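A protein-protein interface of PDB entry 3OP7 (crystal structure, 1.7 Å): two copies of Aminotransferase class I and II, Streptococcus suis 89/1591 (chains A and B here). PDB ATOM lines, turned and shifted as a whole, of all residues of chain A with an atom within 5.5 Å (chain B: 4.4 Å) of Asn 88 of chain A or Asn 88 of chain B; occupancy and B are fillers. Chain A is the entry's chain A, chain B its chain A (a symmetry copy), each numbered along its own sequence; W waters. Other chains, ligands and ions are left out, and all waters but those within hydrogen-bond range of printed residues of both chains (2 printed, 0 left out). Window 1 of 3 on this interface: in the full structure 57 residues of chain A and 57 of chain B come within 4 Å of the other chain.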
ATOM      1  N   GLN A  86     -18.745 -34.255  -9.200  1.00  0.00           N
ATOM      2  CA  GLN A  86     -17.959 -33.521 -10.184  1.00  0.00           C
ATOM      3  C   GLN A  86     -17.863 -32.054  -9.830  1.00  0.00           C
ATOM      4  O   GLN A  86     -18.860 -31.434  -9.388  1.00  0.00           O
ATOM      5  CB  GLN A  86     -18.612 -33.642 -11.564  1.00  0.00           C
ATOM      6  CG  GLN A  86     -17.738 -33.205 -12.721  1.00  0.00           C
ATOM      7  CD  GLN A  86     -18.369 -33.606 -14.026  1.00  0.00           C
ATOM      8  OE1 GLN A  86     -19.317 -32.988 -14.445  1.00  0.00           O
ATOM      9  NE2 GLN A  86     -17.888 -34.657 -14.632  1.00  0.00           N
ATOM     10  N   THR A  87     -16.689 -31.476 -10.110  1.00  0.00           N
ATOM     11  CA  THR A  87     -16.452 -30.073  -9.885  1.00  0.00           C
ATOM     12  C   THR A  87     -15.671 -29.430 -11.025  1.00  0.00           C
ATOM     13  O   THR A  87     -15.122 -30.154 -11.907  1.00  0.00           O
ATOM     14  CB  THR A  87     -15.661 -29.903  -8.576  1.00  0.00           C
ATOM     15  OG1 THR A  87     -14.413 -30.604  -8.709  1.00  0.00           O
ATOM     16  CG2 THR A  87     -16.474 -30.400  -7.348  1.00  0.00           C
ATOM     17  N   ASN A  88     -15.643 -28.094 -11.058  1.00  0.00           N
ATOM     18  CA  ASN A  88     -14.778 -27.384 -12.005  1.00  0.00           C
ATOM     19  C   ASN A  88     -13.327 -27.417 -11.553  1.00  0.00           C
ATOM     20  O   ASN A  88     -12.820 -26.482 -10.901  1.00  0.00           O
ATOM     21  CB  ASN A  88     -15.261 -25.960 -12.313  1.00  0.00           C
ATOM     22  CG  ASN A  88     -15.248 -25.033 -11.100  1.00  0.00           C
ATOM     23  OD1 ASN A  88     -15.704 -25.433 -10.037  1.00  0.00           O
ATOM     24  ND2 ASN A  88     -14.744 -23.780 -11.266  1.00  0.00           N
ATOM     25  N   GLY A  89     -12.628 -28.515 -11.886  1.00  0.00           N
ATOM     26  CA  GLY A  89     -11.279 -28.708 -11.394  1.00  0.00           C
ATOM     27  C   GLY A  89     -11.197 -29.093  -9.943  1.00  0.00           C
ATOM     28  O   GLY A  89     -12.211 -29.013  -9.213  1.00  0.00           O
ATOM     29  N   ALA A  90     -10.004 -29.479  -9.507  1.00  0.00           N
ATOM     30  CA  ALA A  90      -9.691 -29.540  -8.079  1.00  0.00           C
ATOM     31  C   ALA A  90      -9.914 -28.174  -7.391  1.00  0.00           C
ATOM     32  O   ALA A  90     -10.288 -28.131  -6.217  1.00  0.00           O
ATOM     33  CB  ALA A  90      -8.283 -30.089  -7.831  1.00  0.00           C
ATOM     34  N   THR A  91      -9.761 -27.071  -8.150  1.00  0.00           N
ATOM     35  CA  THR A  91     -10.034 -25.723  -7.644  1.00  0.00           C
ATOM     36  C   THR A  91     -11.437 -25.672  -7.049  1.00  0.00           C
ATOM     37  O   THR A  91     -11.643 -25.267  -5.900  1.00  0.00           O
ATOM     38  CB  THR A  91      -9.820 -24.642  -8.727  1.00  0.00           C
ATOM     39  OG1 THR A  91      -8.448 -24.666  -9.207  1.00  0.00           O
ATOM     40  CG2 THR A  91     -10.064 -23.276  -8.152  1.00  0.00           C
ATOM     41  N   GLY A  92     -12.405 -26.061  -7.880  1.00  0.00           N
ATOM     42  CA  GLY A  92     -13.788 -26.021  -7.458  1.00  0.00           C
ATOM     43  C   GLY A  92     -14.094 -26.991  -6.357  1.00  0.00           C
ATOM     44  O   GLY A  92     -14.964 -26.695  -5.491  1.00  0.00           O
ATOM     45  N   ALA A  93     -13.381 -28.129  -6.330  1.00  0.00           N
ATOM     46  CA  ALA A  93     -13.600 -29.129  -5.309  1.00  0.00           C
ATOM     47  C   ALA A  93     -13.107 -28.642  -3.920  1.00  0.00           C
ATOM     48  O   ALA A  93     -13.842 -28.708  -2.926  1.00  0.00           O
ATOM     49  CB  ALA A  93     -12.971 -30.437  -5.632  1.00  0.00           C
ATOM     50  N1  LLP A 222      -4.359 -28.244  -6.196  1.00  0.00           N
ATOM     51  C2  LLP A 222      -2.987 -28.204  -6.427  1.00  0.00           C
ATOM     52  C2' LLP A 222      -2.104 -28.682  -5.313  1.00  0.00           C
ATOM     53  C3  LLP A 222      -2.487 -27.790  -7.663  1.00  0.00           C
ATOM     54  O3  LLP A 222      -1.240 -27.746  -7.857  1.00  0.00           O
ATOM     55  C4  LLP A 222      -3.390 -27.385  -8.686  1.00  0.00           C
ATOM     56  C4' LLP A 222      -2.881 -26.923 -10.029  1.00  0.00           C
ATOM     57  C5  LLP A 222      -4.746 -27.391  -8.403  1.00  0.00           C
ATOM     58  C6  LLP A 222      -5.201 -27.807  -7.188  1.00  0.00           C
ATOM     59  C5' LLP A 222      -5.799 -26.918  -9.401  1.00  0.00           C
ATOM     60  OP4 LLP A 222      -6.228 -27.996 -10.235  1.00  0.00           O
ATOM     61  P   LLP A 222      -7.380 -27.807 -11.314  1.00  0.00           P
ATOM     62  OP1 LLP A 222      -7.908 -29.176 -11.342  1.00  0.00           O
ATOM     63  OP2 LLP A 222      -8.393 -26.898 -10.729  1.00  0.00           O
ATOM     64  OP3 LLP A 222      -6.753 -27.295 -12.567  1.00  0.00           O
ATOM     65  N   LLP A 222      -3.653 -32.409 -13.489  1.00  0.00           N
ATOM     66  CA  LLP A 222      -2.223 -32.494 -13.204  1.00  0.00           C
ATOM     67  CB  LLP A 222      -1.930 -32.115 -11.761  1.00  0.00           C
ATOM     68  CG  LLP A 222      -2.253 -30.642 -11.412  1.00  0.00           C
ATOM     69  CD  LLP A 222      -1.339 -29.657 -12.028  1.00  0.00           C
ATOM     70  CE  LLP A 222      -1.750 -28.170 -11.837  1.00  0.00           C
ATOM     71  NZ  LLP A 222      -1.918 -27.786 -10.412  1.00  0.00           N
ATOM     72  C   LLP A 222      -1.681 -33.866 -13.546  1.00  0.00           C
ATOM     73  O   LLP A 222      -0.709 -33.950 -14.240  1.00  0.00           O
ATOM     74  N   ARG A 230     -11.409 -28.406 -17.195  1.00  0.00           N
ATOM     75  CA  ARG A 230     -11.826 -27.960 -15.883  1.00  0.00           C
ATOM     76  C   ARG A 230     -12.751 -29.036 -15.197  1.00  0.00           C
ATOM     77  O   ARG A 230     -13.914 -28.768 -14.875  1.00  0.00           O
ATOM     78  CB  ARG A 230     -12.496 -26.565 -15.922  1.00  0.00           C
ATOM     79  CG  ARG A 230     -11.831 -25.503 -16.737  1.00  0.00           C
ATOM     80  CD  ARG A 230     -10.391 -25.193 -16.386  1.00  0.00           C
ATOM     81  NE  ARG A 230     -10.202 -24.888 -14.988  1.00  0.00           N
ATOM     82  CZ  ARG A 230      -9.493 -25.600 -14.126  1.00  0.00           C
ATOM     83  NH1 ARG A 230      -8.786 -26.641 -14.522  1.00  0.00           N
ATOM     84  NH2 ARG A 230      -9.418 -25.198 -12.862  1.00  0.00           N
ATOM     85  N   ILE A 231     -12.222 -30.235 -15.017  1.00  0.00           N
ATOM     86  CA  ILE A 231     -12.941 -31.340 -14.373  1.00  0.00           C
ATOM     87  C   ILE A 231     -12.126 -31.903 -13.218  1.00  0.00           C
ATOM     88  O   ILE A 231     -11.043 -32.421 -13.398  1.00  0.00           O
ATOM     89  CB  ILE A 231     -13.283 -32.496 -15.338  1.00  0.00           C
ATOM     90  CG1 ILE A 231     -14.218 -32.037 -16.460  1.00  0.00           C
ATOM     91  CG2 ILE A 231     -13.826 -33.733 -14.593  1.00  0.00           C
ATOM     92  CD1 ILE A 231     -15.676 -31.811 -16.000  1.00  0.00           C
ATOM     93  N   GLY A 232     -12.748 -31.823 -12.054  1.00  0.00           N
ATOM     94  CA  GLY A 232     -12.296 -32.443 -10.849  1.00  0.00           C
ATOM     95  C   GLY A 232     -13.414 -33.156 -10.120  1.00  0.00           C
ATOM     96  O   GLY A 232     -14.536 -33.299 -10.664  1.00  0.00           O
ATOM     97  N   THR A 251     -21.044 -21.723  -6.204  1.00  0.00           N
ATOM     98  CA  THR A 251     -19.733 -21.692  -6.822  1.00  0.00           C
ATOM     99  C   THR A 251     -19.646 -22.101  -8.284  1.00  0.00           C
ATOM    100  O   THR A 251     -18.783 -21.597  -9.010  1.00  0.00           O
ATOM    101  CB  THR A 251     -18.786 -22.592  -5.998  1.00  0.00           C
ATOM    102  OG1 THR A 251     -19.235 -23.946  -6.102  1.00  0.00           O
ATOM    103  CG2 THR A 251     -18.791 -22.113  -4.489  1.00  0.00           C
ATOM    104  N   MET A 252     -20.478 -23.054  -8.739  1.00  0.00           N
ATOM    105  CA  MET A 252     -20.318 -23.601 -10.059  1.00  0.00           C
ATOM    106  C   MET A 252     -21.633 -23.960 -10.790  1.00  0.00           C
ATOM    107  O   MET A 252     -21.669 -23.865 -12.002  1.00  0.00           O
ATOM    108  CB  MET A 252     -19.386 -24.797 -10.017  1.00  0.00           C
ATOM    109  CG  MET A 252     -19.902 -25.895  -9.201  1.00  0.00           C
ATOM    110  SD  MET A 252     -18.882 -27.487  -9.053  1.00  0.00           S
ATOM    111  CE  MET A 252     -17.807 -26.699  -7.619  1.00  0.00           C
ATOM    112  N   ALA A 255     -20.227 -28.528 -13.876  1.00  0.00           N
ATOM    113  CA  ALA A 255     -19.177 -28.404 -14.838  1.00  0.00           C
ATOM    114  C   ALA A 255     -19.743 -28.583 -16.218  1.00  0.00           C
ATOM    115  O   ALA A 255     -20.975 -28.812 -16.376  1.00  0.00           O
ATOM    116  CB  ALA A 255     -18.139 -29.493 -14.558  1.00  0.00           C
ATOM    117  N   THR B  87     -15.486 -16.021 -16.831  1.00  0.00           N
ATOM    118  CA  THR B  87     -15.733 -16.814 -15.654  1.00  0.00           C
ATOM    119  C   THR B  87     -16.504 -18.091 -15.968  1.00  0.00           C
ATOM    120  O   THR B  87     -17.039 -18.246 -17.105  1.00  0.00           O
ATOM    121  CB  THR B  87     -16.540 -15.975 -14.646  1.00  0.00           C
ATOM    122  OG1 THR B  87     -17.783 -15.601 -15.265  1.00  0.00           O
ATOM    123  CG2 THR B  87     -15.738 -14.734 -14.164  1.00  0.00           C
ATOM    124  N   ASN B  88     -16.538 -19.025 -15.013  1.00  0.00           N
ATOM    125  CA  ASN B  88     -17.395 -20.206 -15.148  1.00  0.00           C
ATOM    126  C   ASN B  88     -18.851 -19.860 -14.881  1.00  0.00           C
ATOM    127  O   ASN B  88     -19.371 -20.022 -13.759  1.00  0.00           O
ATOM    128  CB  ASN B  88     -16.916 -21.400 -14.311  1.00  0.00           C
ATOM    129  CG  ASN B  88     -16.948 -21.143 -12.806  1.00  0.00           C
ATOM    130  OD1 ASN B  88     -16.503 -20.090 -12.369  1.00  0.00           O
ATOM    131  ND2 ASN B  88     -17.456 -22.121 -12.007  1.00  0.00           N
ATOM    132  N   GLY B  89     -19.541 -19.359 -15.920  1.00  0.00           N
ATOM    133  CA  GLY B  89     -20.895 -18.874 -15.742  1.00  0.00           C
ATOM    134  C   GLY B  89     -20.992 -17.551 -15.037  1.00  0.00           C
ATOM    135  O   GLY B  89     -19.987 -17.066 -14.469  1.00  0.00           O
ATOM    136  N   ALA B  90     -22.187 -16.974 -15.036  1.00  0.00           N
ATOM    137  CA  ALA B  90     -22.517 -15.890 -14.112  1.00  0.00           C
ATOM    138  C   ALA B  90     -22.309 -16.315 -12.641  1.00  0.00           C
ATOM    139  O   ALA B  90     -21.949 -15.482 -11.805  1.00  0.00           O
ATOM    140  CB  ALA B  90     -23.925 -15.341 -14.361  1.00  0.00           C
ATOM    141  N   THR B  91     -22.459 -17.623 -12.351  1.00  0.00           N
ATOM    142  CA  THR B  91     -22.198 -18.169 -11.017  1.00  0.00           C
ATOM    143  C   THR B  91     -20.802 -17.761 -10.558  1.00  0.00           C
ATOM    144  O   THR B  91     -20.611 -17.195  -9.477  1.00  0.00           O
ATOM    145  CB  THR B  91     -22.405 -19.700 -10.966  1.00  0.00           C
ATOM    146  OG1 THR B  91     -23.771 -20.041 -11.326  1.00  0.00           O
ATOM    147  CG2 THR B  91     -22.174 -20.208  -9.572  1.00  0.00           C
ATOM    148  N   GLY B  92     -19.823 -18.099 -11.398  1.00  0.00           N
ATOM    149  CA  GLY B  92     -18.445 -17.811 -11.065  1.00  0.00           C
ATOM    150  C   GLY B  92     -18.148 -16.343 -11.021  1.00  0.00           C
ATOM    151  O   GLY B  92     -17.288 -15.906 -10.205  1.00  0.00           O
ATOM    152  N   ARG B 230     -20.699 -23.326 -19.471  1.00  0.00           N
ATOM    153  CA  ARG B 230     -20.300 -22.667 -18.246  1.00  0.00           C
ATOM    154  C   ARG B 230     -19.377 -21.428 -18.556  1.00  0.00           C
ATOM    155  O   ARG B 230     -18.219 -21.368 -18.127  1.00  0.00           O
ATOM    156  CB  ARG B 230     -19.636 -23.643 -17.243  1.00  0.00           C
ATOM    157  CG  ARG B 230     -20.298 -24.967 -17.029  1.00  0.00           C
ATOM    158  CD  ARG B 230     -21.743 -24.928 -16.580  1.00  0.00           C
ATOM    159  NE  ARG B 230     -21.950 -24.113 -15.407  1.00  0.00           N
ATOM    160  CZ  ARG B 230     -22.665 -23.001 -15.349  1.00  0.00           C
ATOM    161  NH1 ARG B 230     -23.361 -22.585 -16.388  1.00  0.00           N
ATOM    162  NH2 ARG B 230     -22.757 -22.350 -14.195  1.00  0.00           N
ATOM    163  N   THR B 251     -11.226 -19.784  -6.981  1.00  0.00           N
ATOM    164  CA  THR B 251     -12.530 -20.264  -7.394  1.00  0.00           C
ATOM    165  C   THR B 251     -12.598 -21.057  -8.690  1.00  0.00           C
ATOM    166  O   THR B 251     -13.455 -21.936  -8.826  1.00  0.00           O
ATOM    167  CB  THR B 251     -13.482 -19.054  -7.503  1.00  0.00           C
ATOM    168  OG1 THR B 251     -13.024 -18.205  -8.559  1.00  0.00           O
ATOM    169  CG2 THR B 251     -13.497 -18.275  -6.124  1.00  0.00           C
ATOM    170  N   MET B 252     -11.756 -20.736  -9.688  1.00  0.00           N
ATOM    171  CA  MET B 252     -11.898 -21.331 -10.989  1.00  0.00           C
ATOM    172  C   MET B 252     -10.573 -21.615 -11.735  1.00  0.00           C
ATOM    173  O   MET B 252     -10.523 -22.567 -12.490  1.00  0.00           O
ATOM    174  CB  MET B 252     -12.825 -20.490 -11.847  1.00  0.00           C
ATOM    175  CG  MET B 252     -12.312 -19.142 -12.089  1.00  0.00           C
ATOM    176  SD  MET B 252     -13.325 -17.954 -13.165  1.00  0.00           S
ATOM    177  CE  MET B 252     -14.421 -17.447 -11.625  1.00  0.00           C
HETATM  178  O   HOH W   1     -16.423 -20.173  -9.450  1.00  0.00           O
HETATM  179  O   HOH W   2     -15.817 -23.240  -8.111  1.00  0.00           O
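The backbone carbonyl oxygen of Met 252 of chain B is in hydrogen-bond range of the guanidinium group of Arg 230 of chain A.
O of Thr 251 of chain B lies within hydrogen-bond range of ND2 of Asn 88 of chain A, 3.3 Å away.
The backbone carbonyl oxygen of Thr 251 of chain A is in hydrogen-bond range of the side-chain amide nitrogen of Asn 88 of chain B (3.3 Å).
The backbone carbonyl oxygen (O) of Met 252 of chain A is in hydrogen-bond range of the guanidinium group (NH2) of Arg 230 of chain B (2.9 Å).
The side-chain amide nitrogen (ND2) of Asn 88 of chain B lies close to the side-chain amide nitrogen (ND2) of Asn 88 of chain A, 3.3 Å away.
O of Arg 230 of chain B is in hydrogen-bond range of N of Gly 89 of chain B (3.3 Å).
OP3 of LLP 222 of chain A sits close to the guanidinium group (NH1) of Arg 230 of chain A (2.9 Å).
The side-chain hydroxyl of Thr 91 of chain A sits close to OP2 of LLP 222 of chain A, 2.7 Å away.
The backbone carbonyl oxygen (O) of Arg 230 of chain A lies within hydrogen-bond range of the backbone NH (N) of Gly 89 of chain A (3.3 Å).
Among the printed residues, merely in contact across the chains: Thr 251 of chain A with Thr 91 of chain B, Thr 91 of chain A with Thr 251 of chain B, Met 252 of chain A with Thr 91 of chain B, Thr 91 of chain A with Met 252 of chain B, Ala 255 of chain A with Arg 230 of chain B, Asn 88 of chain A with Met 252 of chain B and Met 252 of chain A with Asn 88 of chain B.
Asn 88 of chain A touches three residues of chain B.
Of the printed residues of chain A, Asn 88 of chain B touches Asn 88, Thr 251 and Met 252.
Of the printed residues of chain A, Arg 230 of chain B touches Met 252 and Ala 255.
Of the printed residues of chain A, Met 252 of chain B touches Asn 88, Thr 91 and Arg 230.
The nearest printed residue of chain A that does not touch Asn 88 of chain B is Arg 230 of chain A (7.0 Å).
The nearest printed residue of chain A that does not touch Thr 91 of chain B is Asn 88 of chain A (8.3 Å).
Of the 15 printed residues of chain A, 6 touch a printed residue of chain B.
Of the 9 printed residues of chain B, 5 touch a printed residue of chain A.
Hydrophobic or aromatic side chains of chain B that line the printed part of chain A: Met 252.
Along chain B the printed residues that touch a printed residue of chain A span positions 88 to 252.
Among the printed residues, 12 pairs touch across the chains.
Among the printed residues, no Asp or Glu carboxylate lies within 4 Å of a Lys or Arg side-chain nitrogen of the other chain.
Asn 88 of chain A touches its own counterpart, Asn 88 of chain B.
Thr 91 of chain A touches Thr 251 of chain B, and with the chains exchanged Thr 251 of chain A touches Thr 91 of chain B.
Thr 91 of chain A touches Met 252 of chain B, and with the chains exchanged Met 252 of chain A touches Thr 91 of chain B.
Arg 230 of chain A touches Met 252 of chain B, and with the chains exchanged Met 252 of chain A touches Arg 230 of chain B.
9 positions are printed for both chains.
Of the 12 pairs that touch across the chains among the printed residues, 11 have their exchanged pair printed and touching as well.
Water W2 lies within hydrogen-bond range of O of Thr 251 of chain B and OD1 of Asn 88 of chain A.
Water W1 lies within hydrogen-bond range of O of Thr 251 of chain A (2.8 Å) and OD1 of Asn 88 of chain B (2.9 Å).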
